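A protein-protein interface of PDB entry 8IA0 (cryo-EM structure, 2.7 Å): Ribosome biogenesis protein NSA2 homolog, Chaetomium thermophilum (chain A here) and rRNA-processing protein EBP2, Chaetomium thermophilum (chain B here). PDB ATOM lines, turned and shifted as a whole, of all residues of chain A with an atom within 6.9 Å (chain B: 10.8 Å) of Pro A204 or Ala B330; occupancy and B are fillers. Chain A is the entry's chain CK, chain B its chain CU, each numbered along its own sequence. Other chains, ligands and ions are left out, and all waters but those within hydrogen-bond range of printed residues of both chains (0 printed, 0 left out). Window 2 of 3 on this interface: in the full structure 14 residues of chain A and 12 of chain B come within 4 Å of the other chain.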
ATOM      1  N   LYS A 202     -36.186  14.768 -16.430  1.00  0.00           N
ATOM      2  CA  LYS A 202     -35.159  13.854 -15.947  1.00  0.00           C
ATOM      3  C   LYS A 202     -34.846  14.142 -14.488  1.00  0.00           C
ATOM      4  O   LYS A 202     -34.545  15.283 -14.126  1.00  0.00           O
ATOM      5  CB  LYS A 202     -33.884  13.957 -16.789  1.00  0.00           C
ATOM      6  CG  LYS A 202     -32.875  12.860 -16.504  1.00  0.00           C
ATOM      7  CD  LYS A 202     -31.464  13.309 -16.822  1.00  0.00           C
ATOM      8  CE  LYS A 202     -30.466  12.200 -16.558  1.00  0.00           C
ATOM      9  NZ  LYS A 202     -30.961  10.888 -17.049  1.00  0.00           N
ATOM     10  N   ASN A 203     -34.911  13.100 -13.661  1.00  0.00           N
ATOM     11  CA  ASN A 203     -34.470  13.171 -12.280  1.00  0.00           C
ATOM     12  C   ASN A 203     -33.141  12.443 -12.178  1.00  0.00           C
ATOM     13  O   ASN A 203     -33.119  11.206 -12.256  1.00  0.00           O
ATOM     14  CB  ASN A 203     -35.502  12.539 -11.350  1.00  0.00           C
ATOM     15  CG  ASN A 203     -35.293  12.912  -9.896  1.00  0.00           C
ATOM     16  OD1 ASN A 203     -36.056  12.499  -9.027  1.00  0.00           O
ATOM     17  ND2 ASN A 203     -34.260  13.699  -9.625  1.00  0.00           N
ATOM     18  N   PRO A 204     -32.020  13.142 -12.010  1.00  0.00           N
ATOM     19  CA  PRO A 204     -30.695  12.514 -12.084  1.00  0.00           C
ATOM     20  C   PRO A 204     -30.314  11.720 -10.838  1.00  0.00           C
ATOM     21  O   PRO A 204     -29.164  11.728 -10.401  1.00  0.00           O
ATOM     22  CB  PRO A 204     -29.761  13.712 -12.285  1.00  0.00           C
ATOM     23  CG  PRO A 204     -30.645  14.878 -12.601  1.00  0.00           C
ATOM     24  CD  PRO A 204     -31.917  14.601 -11.889  1.00  0.00           C
ATOM     25  N   SER A 205     -31.286  11.026 -10.265  1.00  0.00           N
ATOM     26  CA  SER A 205     -31.031  10.138  -9.137  1.00  0.00           C
ATOM     27  C   SER A 205     -31.596   8.741  -9.321  1.00  0.00           C
ATOM     28  O   SER A 205     -31.059   7.800  -8.728  1.00  0.00           O
ATOM     29  CB  SER A 205     -31.603  10.734  -7.846  1.00  0.00           C
ATOM     30  OG  SER A 205     -30.993  11.972  -7.535  1.00  0.00           O
ATOM     31  N   ASN A 206     -32.640   8.566 -10.118  1.00  0.00           N
ATOM     32  CA  ASN A 206     -33.291   7.282 -10.293  1.00  0.00           C
ATOM     33  C   ASN A 206     -34.205   7.399 -11.507  1.00  0.00           C
ATOM     34  O   ASN A 206     -35.071   8.283 -11.540  1.00  0.00           O
ATOM     35  CB  ASN A 206     -34.067   6.917  -9.025  1.00  0.00           C
ATOM     36  CG  ASN A 206     -34.514   5.468  -8.989  1.00  0.00           C
ATOM     37  OD1 ASN A 206     -34.570   4.811 -10.027  1.00  0.00           O
ATOM     38  ND2 ASN A 206     -34.840   4.962  -7.809  1.00  0.00           N
ATOM     39  N   PRO A 207     -34.038   6.551 -12.524  1.00  0.00           N
ATOM     40  CA  PRO A 207     -34.983   6.581 -13.652  1.00  0.00           C
ATOM     41  C   PRO A 207     -36.417   6.327 -13.235  1.00  0.00           C
ATOM     42  O   PRO A 207     -37.342   6.835 -13.880  1.00  0.00           O
ATOM     43  CB  PRO A 207     -34.455   5.476 -14.576  1.00  0.00           C
ATOM     44  CG  PRO A 207     -33.010   5.376 -14.245  1.00  0.00           C
ATOM     45  CD  PRO A 207     -32.906   5.647 -12.775  1.00  0.00           C
ATOM     46  N   THR A 210     -38.064   9.627 -12.292  1.00  0.00           N
ATOM     47  CA  THR A 210     -38.513  10.407 -13.439  1.00  0.00           C
ATOM     48  C   THR A 210     -39.893   9.956 -13.897  1.00  0.00           C
ATOM     49  O   THR A 210     -40.768  10.785 -14.176  1.00  0.00           O
ATOM     50  CB  THR A 210     -37.503  10.291 -14.579  1.00  0.00           C
ATOM     51  OG1 THR A 210     -36.387  11.149 -14.319  1.00  0.00           O
ATOM     52  CG2 THR A 210     -38.136  10.695 -15.899  1.00  0.00           C
ATOM     53  N   THR A 216     -36.830  16.296  -6.990  1.00  0.00           N
ATOM     54  CA  THR A 216     -35.702  16.431  -6.082  1.00  0.00           C
ATOM     55  C   THR A 216     -34.779  17.535  -6.585  1.00  0.00           C
ATOM     56  O   THR A 216     -35.037  18.175  -7.607  1.00  0.00           O
ATOM     57  CB  THR A 216     -34.944  15.108  -5.943  1.00  0.00           C
ATOM     58  OG1 THR A 216     -34.489  14.675  -7.231  1.00  0.00           O
ATOM     59  CG2 THR A 216     -35.837  14.042  -5.337  1.00  0.00           C
ATOM     60  N   LYS A 217     -33.694  17.758  -5.852  1.00  0.00           N
ATOM     61  CA  LYS A 217     -32.728  18.772  -6.241  1.00  0.00           C
ATOM     62  C   LYS A 217     -31.993  18.350  -7.508  1.00  0.00           C
ATOM     63  O   LYS A 217     -31.575  17.198  -7.650  1.00  0.00           O
ATOM     64  CB  LYS A 217     -31.733  19.019  -5.108  1.00  0.00           C
ATOM     65  CG  LYS A 217     -30.535  19.865  -5.495  1.00  0.00           C
ATOM     66  CD  LYS A 217     -29.565  20.018  -4.338  1.00  0.00           C
ATOM     67  CE  LYS A 217     -30.033  21.078  -3.357  1.00  0.00           C
ATOM     68  NZ  LYS A 217     -30.452  22.325  -4.052  1.00  0.00           N
ATOM     69  N   GLY A 218     -31.837  19.292  -8.432  1.00  0.00           N
ATOM     70  CA  GLY A 218     -31.149  19.008  -9.679  1.00  0.00           C
ATOM     71  C   GLY A 218     -32.008  18.328 -10.722  1.00  0.00           C
ATOM     72  O   GLY A 218     -31.482  17.817 -11.718  1.00  0.00           O
ATOM     73  N   THR A 219     -33.323  18.329 -10.529  1.00  0.00           N
ATOM     74  CA  THR A 219     -34.258  17.699 -11.448  1.00  0.00           C
ATOM     75  C   THR A 219     -34.637  18.685 -12.542  1.00  0.00           C
ATOM     76  O   THR A 219     -34.953  19.844 -12.257  1.00  0.00           O
ATOM     77  CB  THR A 219     -35.514  17.224 -10.715  1.00  0.00           C
ATOM     78  OG1 THR A 219     -35.136  16.418  -9.592  1.00  0.00           O
ATOM     79  CG2 THR A 219     -36.398  16.412 -11.639  1.00  0.00           C
ATOM     80  N   ILE A 220     -34.601  18.224 -13.788  1.00  0.00           N
ATOM     81  CA  ILE A 220     -34.976  19.054 -14.927  1.00  0.00           C
ATOM     82  C   ILE A 220     -36.476  18.933 -15.151  1.00  0.00           C
ATOM     83  O   ILE A 220     -37.001  17.831 -15.332  1.00  0.00           O
ATOM     84  CB  ILE A 220     -34.197  18.655 -16.185  1.00  0.00           C
ATOM     85  CG1 ILE A 220     -32.712  18.966 -16.014  1.00  0.00           C
ATOM     86  CG2 ILE A 220     -34.759  19.366 -17.402  1.00  0.00           C
ATOM     87  CD1 ILE A 220     -32.406  20.440 -15.952  1.00  0.00           C
ATOM     88  N   GLN A 244     -34.192  23.783 -13.941  1.00  0.00           N
ATOM     89  CA  GLN A 244     -33.583  22.866 -12.986  1.00  0.00           C
ATOM     90  C   GLN A 244     -33.966  23.277 -11.570  1.00  0.00           C
ATOM     91  O   GLN A 244     -33.789  24.437 -11.188  1.00  0.00           O
ATOM     92  CB  GLN A 244     -32.064  22.841 -13.139  1.00  0.00           C
ATOM     93  CG  GLN A 244     -31.358  22.076 -12.038  1.00  0.00           C
ATOM     94  CD  GLN A 244     -30.071  21.432 -12.497  1.00  0.00           C
ATOM     95  OE1 GLN A 244     -30.032  20.241 -12.797  1.00  0.00           O
ATOM     96  NE2 GLN A 244     -29.005  22.221 -12.562  1.00  0.00           N
ATOM     97  N   GLU B 322     -21.183   2.741  -8.989  1.00  0.00           N
ATOM     98  CA  GLU B 322     -21.598   3.011 -10.362  1.00  0.00           C
ATOM     99  C   GLU B 322     -22.796   3.951 -10.408  1.00  0.00           C
ATOM    100  O   GLU B 322     -22.855   4.850 -11.254  1.00  0.00           O
ATOM    101  CB  GLU B 322     -21.917   1.700 -11.079  1.00  0.00           C
ATOM    102  CG  GLU B 322     -22.157   1.854 -12.568  1.00  0.00           C
ATOM    103  CD  GLU B 322     -23.018   0.745 -13.139  1.00  0.00           C
ATOM    104  OE1 GLU B 322     -23.680   0.039 -12.350  1.00  0.00           O
ATOM    105  OE2 GLU B 322     -23.032   0.578 -14.377  1.00  0.00           O
ATOM    106  N   ARG B 323     -23.765   3.758  -9.509  1.00  0.00           N
ATOM    107  CA  ARG B 323     -24.935   4.630  -9.487  1.00  0.00           C
ATOM    108  C   ARG B 323     -24.554   6.062  -9.137  1.00  0.00           C
ATOM    109  O   ARG B 323     -25.125   7.013  -9.682  1.00  0.00           O
ATOM    110  CB  ARG B 323     -25.978   4.097  -8.506  1.00  0.00           C
ATOM    111  CG  ARG B 323     -26.980   3.139  -9.122  1.00  0.00           C
ATOM    112  CD  ARG B 323     -27.243   1.946  -8.230  1.00  0.00           C
ATOM    113  NE  ARG B 323     -28.178   1.014  -8.848  1.00  0.00           N
ATOM    114  CZ  ARG B 323     -29.149   0.386  -8.199  1.00  0.00           C
ATOM    115  NH1 ARG B 323     -29.346   0.569  -6.904  1.00  0.00           N
ATOM    116  NH2 ARG B 323     -29.941  -0.446  -8.867  1.00  0.00           N
ATOM    117  N   ALA B 324     -23.597   6.236  -8.223  1.00  0.00           N
ATOM    118  CA  ALA B 324     -23.105   7.576  -7.921  1.00  0.00           C
ATOM    119  C   ALA B 324     -22.413   8.191  -9.129  1.00  0.00           C
ATOM    120  O   ALA B 324     -22.548   9.392  -9.386  1.00  0.00           O
ATOM    121  CB  ALA B 324     -22.158   7.529  -6.724  1.00  0.00           C
ATOM    122  N   LYS B 325     -21.659   7.384  -9.878  1.00  0.00           N
ATOM    123  CA  LYS B 325     -20.994   7.889 -11.075  1.00  0.00           C
ATOM    124  C   LYS B 325     -22.005   8.341 -12.119  1.00  0.00           C
ATOM    125  O   LYS B 325     -21.827   9.385 -12.755  1.00  0.00           O
ATOM    126  CB  LYS B 325     -20.066   6.821 -11.650  1.00  0.00           C
ATOM    127  CG  LYS B 325     -19.269   7.280 -12.855  1.00  0.00           C
ATOM    128  CD  LYS B 325     -18.894   6.110 -13.746  1.00  0.00           C
ATOM    129  CE  LYS B 325     -17.692   5.361 -13.199  1.00  0.00           C
ATOM    130  NZ  LYS B 325     -16.813   6.239 -12.379  1.00  0.00           N
ATOM    131  N   GLN B 326     -23.079   7.569 -12.308  1.00  0.00           N
ATOM    132  CA  GLN B 326     -24.113   7.959 -13.261  1.00  0.00           C
ATOM    133  C   GLN B 326     -24.771   9.271 -12.854  1.00  0.00           C
ATOM    134  O   GLN B 326     -25.174  10.065 -13.711  1.00  0.00           O
ATOM    135  CB  GLN B 326     -25.159   6.851 -13.385  1.00  0.00           C
ATOM    136  CG  GLN B 326     -24.615   5.540 -13.919  1.00  0.00           C
ATOM    137  CD  GLN B 326     -25.687   4.481 -14.056  1.00  0.00           C
ATOM    138  OE1 GLN B 326     -26.767   4.597 -13.477  1.00  0.00           O
ATOM    139  NE2 GLN B 326     -25.395   3.438 -14.824  1.00  0.00           N
ATOM    140  N   LYS B 327     -24.897   9.509 -11.549  1.00  0.00           N
ATOM    141  CA  LYS B 327     -25.422  10.783 -11.072  1.00  0.00           C
ATOM    142  C   LYS B 327     -24.508  11.933 -11.473  1.00  0.00           C
ATOM    143  O   LYS B 327     -24.975  13.006 -11.872  1.00  0.00           O
ATOM    144  CB  LYS B 327     -25.598  10.734  -9.554  1.00  0.00           C
ATOM    145  CG  LYS B 327     -26.487  11.822  -8.991  1.00  0.00           C
ATOM    146  CD  LYS B 327     -26.797  11.580  -7.525  1.00  0.00           C
ATOM    147  CE  LYS B 327     -27.274  12.849  -6.844  1.00  0.00           C
ATOM    148  NZ  LYS B 327     -28.069  13.704  -7.766  1.00  0.00           N
ATOM    149  N   ARG B 328     -23.196  11.725 -11.368  1.00  0.00           N
ATOM    150  CA  ARG B 328     -22.248  12.784 -11.691  1.00  0.00           C
ATOM    151  C   ARG B 328     -22.268  13.120 -13.178  1.00  0.00           C
ATOM    152  O   ARG B 328     -22.241  14.297 -13.554  1.00  0.00           O
ATOM    153  CB  ARG B 328     -20.845  12.373 -11.249  1.00  0.00           C
ATOM    154  CG  ARG B 328     -20.259  13.254 -10.163  1.00  0.00           C
ATOM    155  CD  ARG B 328     -18.816  12.887  -9.860  1.00  0.00           C
ATOM    156  NE  ARG B 328     -18.701  11.554  -9.282  1.00  0.00           N
ATOM    157  CZ  ARG B 328     -18.259  10.488  -9.933  1.00  0.00           C
ATOM    158  NH1 ARG B 328     -17.877  10.559 -11.197  1.00  0.00           N
ATOM    159  NH2 ARG B 328     -18.197   9.321  -9.298  1.00  0.00           N
ATOM    160  N   GLU B 329     -22.310  12.101 -14.041  1.00  0.00           N
ATOM    161  CA  GLU B 329     -22.332  12.355 -15.478  1.00  0.00           C
ATOM    162  C   GLU B 329     -23.610  13.069 -15.898  1.00  0.00           C
ATOM    163  O   GLU B 329     -23.577  13.971 -16.742  1.00  0.00           O
ATOM    164  CB  GLU B 329     -22.169  11.047 -16.252  1.00  0.00           C
ATOM    165  CG  GLU B 329     -21.135  10.100 -15.676  1.00  0.00           C
ATOM    166  CD  GLU B 329     -20.480   9.237 -16.736  1.00  0.00           C
ATOM    167  OE1 GLU B 329     -20.564   9.592 -17.930  1.00  0.00           O
ATOM    168  OE2 GLU B 329     -19.882   8.201 -16.375  1.00  0.00           O
ATOM    169  N   ALA B 330     -24.749  12.670 -15.328  1.00  0.00           N
ATOM    170  CA  ALA B 330     -26.011  13.316 -15.670  1.00  0.00           C
ATOM    171  C   ALA B 330     -26.004  14.786 -15.276  1.00  0.00           C
ATOM    172  O   ALA B 330     -26.476  15.641 -16.033  1.00  0.00           O
ATOM    173  CB  ALA B 330     -27.172  12.586 -14.998  1.00  0.00           C
ATOM    174  N   LEU B 331     -25.476  15.101 -14.092  1.00  0.00           N
ATOM    175  CA  LEU B 331     -25.404  16.492 -13.662  1.00  0.00           C
ATOM    176  C   LEU B 331     -24.400  17.275 -14.499  1.00  0.00           C
ATOM    177  O   LEU B 331     -24.584  18.473 -14.743  1.00  0.00           O
ATOM    178  CB  LEU B 331     -25.045  16.566 -12.178  1.00  0.00           C
ATOM    179  CG  LEU B 331     -26.088  16.041 -11.188  1.00  0.00           C
ATOM    180  CD1 LEU B 331     -25.543  16.077  -9.771  1.00  0.00           C
ATOM    181  CD2 LEU B 331     -27.377  16.835 -11.285  1.00  0.00           C
ATOM    182  N   ASP B 332     -23.326  16.615 -14.940  1.00  0.00           N
ATOM    183  CA  ASP B 332     -22.341  17.277 -15.788  1.00  0.00           C
ATOM    184  C   ASP B 332     -22.968  17.673 -17.121  1.00  0.00           C
ATOM    185  O   ASP B 332     -22.793  18.806 -17.585  1.00  0.00           O
ATOM    186  CB  ASP B 332     -21.133  16.344 -15.968  1.00  0.00           C
ATOM    187  CG  ASP B 332     -20.118  16.820 -17.019  1.00  0.00           C
ATOM    188  OD1 ASP B 332     -20.351  17.784 -17.775  1.00  0.00           O
ATOM    189  OD2 ASP B 332     -19.040  16.192 -17.082  1.00  0.00           O
ATOM    190  N   LYS B 333     -23.726  16.762 -17.736  1.00  0.00           N
ATOM    191  CA  LYS B 333     -24.359  17.066 -19.015  1.00  0.00           C
ATOM    192  C   LYS B 333     -25.376  18.191 -18.875  1.00  0.00           C
ATOM    193  O   LYS B 333     -25.485  19.052 -19.756  1.00  0.00           O
ATOM    194  CB  LYS B 333     -25.019  15.814 -19.588  1.00  0.00           C
ATOM    195  CG  LYS B 333     -24.035  14.776 -20.102  1.00  0.00           C
ATOM    196  CD  LYS B 333     -24.745  13.648 -20.836  1.00  0.00           C
ATOM    197  CE  LYS B 333     -25.341  14.113 -22.157  1.00  0.00           C
ATOM    198  NZ  LYS B 333     -24.613  15.272 -22.742  1.00  0.00           N
ATOM    199  N   ILE B 334     -26.136  18.195 -17.780  1.00  0.00           N
ATOM    200  CA  ILE B 334     -27.058  19.299 -17.521  1.00  0.00           C
ATOM    201  C   ILE B 334     -26.288  20.599 -17.340  1.00  0.00           C
ATOM    202  O   ILE B 334     -26.677  21.649 -17.866  1.00  0.00           O
ATOM    203  CB  ILE B 334     -27.936  18.984 -16.296  1.00  0.00           C
ATOM    204  CG1 ILE B 334     -28.877  17.818 -16.597  1.00  0.00           C
ATOM    205  CG2 ILE B 334     -28.724  20.211 -15.875  1.00  0.00           C
ATOM    206  CD1 ILE B 334     -29.446  17.164 -15.359  1.00  0.00           C
ATOM    207  N   ASN B 335     -25.182  20.550 -16.594  1.00  0.00           N
ATOM    208  CA  ASN B 335     -24.388  21.750 -16.357  1.00  0.00           C
ATOM    209  C   ASN B 335     -23.732  22.224 -17.651  1.00  0.00           C
ATOM    210  O   ASN B 335     -23.573  23.430 -17.866  1.00  0.00           O
ATOM    211  CB  ASN B 335     -23.346  21.462 -15.271  1.00  0.00           C
ATOM    212  CG  ASN B 335     -22.545  22.693 -14.849  1.00  0.00           C
ATOM    213  OD1 ASN B 335     -22.591  23.718 -15.525  1.00  0.00           O
ATOM    214  ND2 ASN B 335     -21.773  22.584 -13.777  1.00  0.00           N
ATOM    215  N   GLN B 336     -23.335  21.289 -18.519  1.00  0.00           N
ATOM    216  CA  GLN B 336     -22.778  21.671 -19.812  1.00  0.00           C
ATOM    217  C   GLN B 336     -23.813  22.386 -20.668  1.00  0.00           C
ATOM    218  O   GLN B 336     -23.491  23.349 -21.372  1.00  0.00           O
ATOM    219  CB  GLN B 336     -22.244  20.438 -20.541  1.00  0.00           C
ATOM    220  CG  GLN B 336     -20.772  20.171 -20.308  1.00  0.00           C
ATOM    221  CD  GLN B 336     -20.225  19.108 -21.233  1.00  0.00           C
ATOM    222  OE1 GLN B 336     -20.890  18.112 -21.515  1.00  0.00           O
ATOM    223  NE2 GLN B 336     -19.006  19.314 -21.717  1.00  0.00           N
ATOM    224  N   LEU B 337     -25.062  21.919 -20.629  1.00  0.00           N
ATOM    225  CA  LEU B 337     -26.130  22.595 -21.355  1.00  0.00           C
ATOM    226  C   LEU B 337     -26.355  24.000 -20.815  1.00  0.00           C
ATOM    227  O   LEU B 337     -26.663  24.925 -21.575  1.00  0.00           O
ATOM    228  CB  LEU B 337     -27.415  21.776 -21.270  1.00  0.00           C
ATOM    229  CG  LEU B 337     -28.532  22.158 -22.236  1.00  0.00           C
ATOM    230  CD1 LEU B 337     -28.256  21.572 -23.605  1.00  0.00           C
ATOM    231  CD2 LEU B 337     -29.878  21.689 -21.715  1.00  0.00           C
ATOM    232  N   LYS B 338     -26.212  24.177 -19.499  1.00  0.00           N
ATOM    233  CA  LYS B 338     -26.395  25.493 -18.899  1.00  0.00           C
ATOM    234  C   LYS B 338     -25.378  26.493 -19.434  1.00  0.00           C
ATOM    235  O   LYS B 338     -25.723  27.642 -19.730  1.00  0.00           O
ATOM    236  CB  LYS B 338     -26.295  25.389 -17.378  1.00  0.00           C
ATOM    237  CG  LYS B 338     -27.633  25.257 -16.677  1.00  0.00           C
ATOM    238  CD  LYS B 338     -27.536  25.613 -15.200  1.00  0.00           C
ATOM    239  CE  LYS B 338     -26.492  26.685 -14.943  1.00  0.00           C
ATOM    240  NZ  LYS B 338     -26.657  27.301 -13.599  1.00  0.00           N
ATOM    241  N   ARG B 339     -24.115  26.077 -19.555  1.00  0.00           N
ATOM    242  CA  ARG B 339     -23.094  26.968 -20.098  1.00  0.00           C
ATOM    243  C   ARG B 339     -23.370  27.303 -21.556  1.00  0.00           C
ATOM    244  O   ARG B 339     -23.212  28.454 -21.977  1.00  0.00           O
ATOM    245  CB  ARG B 339     -21.709  26.336 -19.955  1.00  0.00           C
ATOM    246  CG  ARG B 339     -20.909  26.830 -18.763  1.00  0.00           C
ATOM    247  CD  ARG B 339     -21.189  25.996 -17.532  1.00  0.00           C
ATOM    248  NE  ARG B 339     -20.888  24.587 -17.756  1.00  0.00           N
ATOM    249  CZ  ARG B 339     -19.684  24.047 -17.625  1.00  0.00           C
ATOM    250  NH1 ARG B 339     -18.637  24.771 -17.268  1.00  0.00           N
ATOM    251  NH2 ARG B 339     -19.527  22.746 -17.857  1.00  0.00           N
ATOM    252  N   PHE B 358     -35.022  13.288 -22.900  1.00  0.00           N
ATOM    253  CA  PHE B 358     -33.968  14.189 -22.435  1.00  0.00           C
ATOM    254  C   PHE B 358     -32.632  13.465 -22.294  1.00  0.00           C
ATOM    255  O   PHE B 358     -31.931  13.577 -21.291  1.00  0.00           O
ATOM    256  CB  PHE B 358     -34.389  14.824 -21.114  1.00  0.00           C
ATOM    257  CG  PHE B 358     -33.585  16.035 -20.728  1.00  0.00           C
ATOM    258  CD1 PHE B 358     -33.798  17.251 -21.349  1.00  0.00           C
ATOM    259  CD2 PHE B 358     -32.631  15.962 -19.727  1.00  0.00           C
ATOM    260  CE1 PHE B 358     -33.065  18.365 -20.990  1.00  0.00           C
ATOM    261  CE2 PHE B 358     -31.896  17.070 -19.367  1.00  0.00           C
ATOM    262  CZ  PHE B 358     -32.114  18.273 -19.998  1.00  0.00           C
ATOM    263  N   ASP B 359     -32.281  12.699 -23.299  1.00  0.00           N
ATOM    264  CA  ASP B 359     -30.910  12.249 -23.498  1.00  0.00           C
ATOM    265  C   ASP B 359     -30.455  12.443 -24.933  1.00  0.00           C
ATOM    266  O   ASP B 359     -29.301  12.810 -25.166  1.00  0.00           O
ATOM    267  CB  ASP B 359     -30.763  10.778 -23.089  1.00  0.00           C
ATOM    268  CG  ASP B 359     -30.559  10.611 -21.597  1.00  0.00           C
ATOM    269  OD1 ASP B 359     -29.828  11.430 -21.001  1.00  0.00           O
ATOM    270  OD2 ASP B 359     -31.127   9.661 -21.019  1.00  0.00           O
ATOM    271  N   VAL B 362     -30.463  16.472 -25.491  1.00  0.00           N
ATOM    272  CA  VAL B 362     -29.257  17.115 -24.983  1.00  0.00           C
ATOM    273  C   VAL B 362     -28.058  16.761 -25.851  1.00  0.00           C
ATOM    274  O   VAL B 362     -27.210  17.613 -26.142  1.00  0.00           O
ATOM    275  CB  VAL B 362     -29.028  16.728 -23.513  1.00  0.00           C
ATOM    276  CG1 VAL B 362     -27.852  17.499 -22.939  1.00  0.00           C
ATOM    277  CG2 VAL B 362     -30.283  16.979 -22.705  1.00  0.00           C
ATOM    278  N   ASP B 363     -27.964  15.498 -26.275  1.00  0.00           N
ATOM    279  CA  ASP B 363     -26.856  15.086 -27.132  1.00  0.00           C
ATOM    280  C   ASP B 363     -26.894  15.814 -28.469  1.00  0.00           C
ATOM    281  O   ASP B 363     -25.852  16.236 -28.983  1.00  0.00           O
ATOM    282  CB  ASP B 363     -26.893  13.573 -27.342  1.00  0.00           C
ATOM    283  CG  ASP B 363     -26.183  12.814 -26.241  1.00  0.00           C
ATOM    284  OD1 ASP B 363     -25.302  13.405 -25.582  1.00  0.00           O
ATOM    285  OD2 ASP B 363     -26.504  11.626 -26.034  1.00  0.00           O
ATOM    286  N   LEU B 366     -25.916  19.675 -27.828  1.00  0.00           N
ATOM    287  CA  LEU B 366     -24.491  19.852 -27.580  1.00  0.00           C
ATOM    288  C   LEU B 366     -23.645  19.511 -28.799  1.00  0.00           C
ATOM    289  O   LEU B 366     -22.503  19.974 -28.895  1.00  0.00           O
ATOM    290  CB  LEU B 366     -24.052  19.002 -26.387  1.00  0.00           C
ATOM    291  CG  LEU B 366     -24.549  19.460 -25.016  1.00  0.00           C
ATOM    292  CD1 LEU B 366     -24.294  18.395 -23.966  1.00  0.00           C
ATOM    293  CD2 LEU B 366     -23.889  20.769 -24.622  1.00  0.00           C
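O of Pro A204 lies close to NZ of Lys B327 (3.5 Å).
NZ of Lys B327 sits at hydrogen-bond distance from OG of Ser A205 (3.4 Å).
The backbone carbonyl oxygen (O) of Lys A202 lies within hydrogen-bond range of the backbone NH (N) of Ile A220 (3.0 Å).
The backbone carbonyl oxygen (O) of Gly A218 sits close to the side-chain amide oxygen (OE1) of Gln A244 (3.0 Å).
Among the printed residues, pairs that only touch across the chains: Gln A244 with Ile B334, Lys A202 with Ala B330, Ile A220 with Ile B334, Lys A202 with Phe B358, Pro A204 with Ile B334, Ile A220 with Phe B358 and Pro A204 with Ala B330.
Of the printed residues of chain B, Lys A202 touches Ala B330 and Phe B358.
No residue of chain B comes within 4 Å of Asn A203.
Pro A204 touches just these residues of chain B: Lys B327, Ala B330 and Ile B334.
No residue of chain B comes within 4 Å of Gly A218.
No residue of chain B comes within 4 Å of Thr A219.
Of the printed residues of chain B, Ile A220 touches Ile B334 (3.7 Å) and Phe B358 (3.9 Å).
Printed residues of chain B within 4 Å of Gln A244: Ile B334.
Arg B323 touches none of the printed residues of chain A.
Of the printed residues of chain A, Lys B327 touches Pro A204 and Ser A205.
Of chain A, only Lys A202 (3.7 Å) and Pro A204 (3.9 Å) come within 4 Å of Ala B330.
Of the printed residues of chain A, Ile B334 touches Pro A204 (3.8 Å), Ile A220 (3.7 Å) and Gln A244 (3.3 Å).
Of the printed residues of chain A, Phe B358 touches Lys A202 (3.8 Å) and Ile A220 (3.9 Å).
The nearest residue of chain A that does not touch Ala B330 is Ser A205 (6.5 Å).
Printed residues of chain B that touch a printed residue of chain A: Lys B327, Ala B330, Ile B334 and Phe B358.
Hydrophobic or aromatic side chains of chain B within 4 Å of the printed part of chain A: Ala B330, Ile B334 and Phe B358.
Of the 13 printed residues of chain A, 5 touch a printed residue of chain B.
Hydrophobic or aromatic side chains of chain A within 4 Å of the printed part of chain B: Pro A204 and Ile A220.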
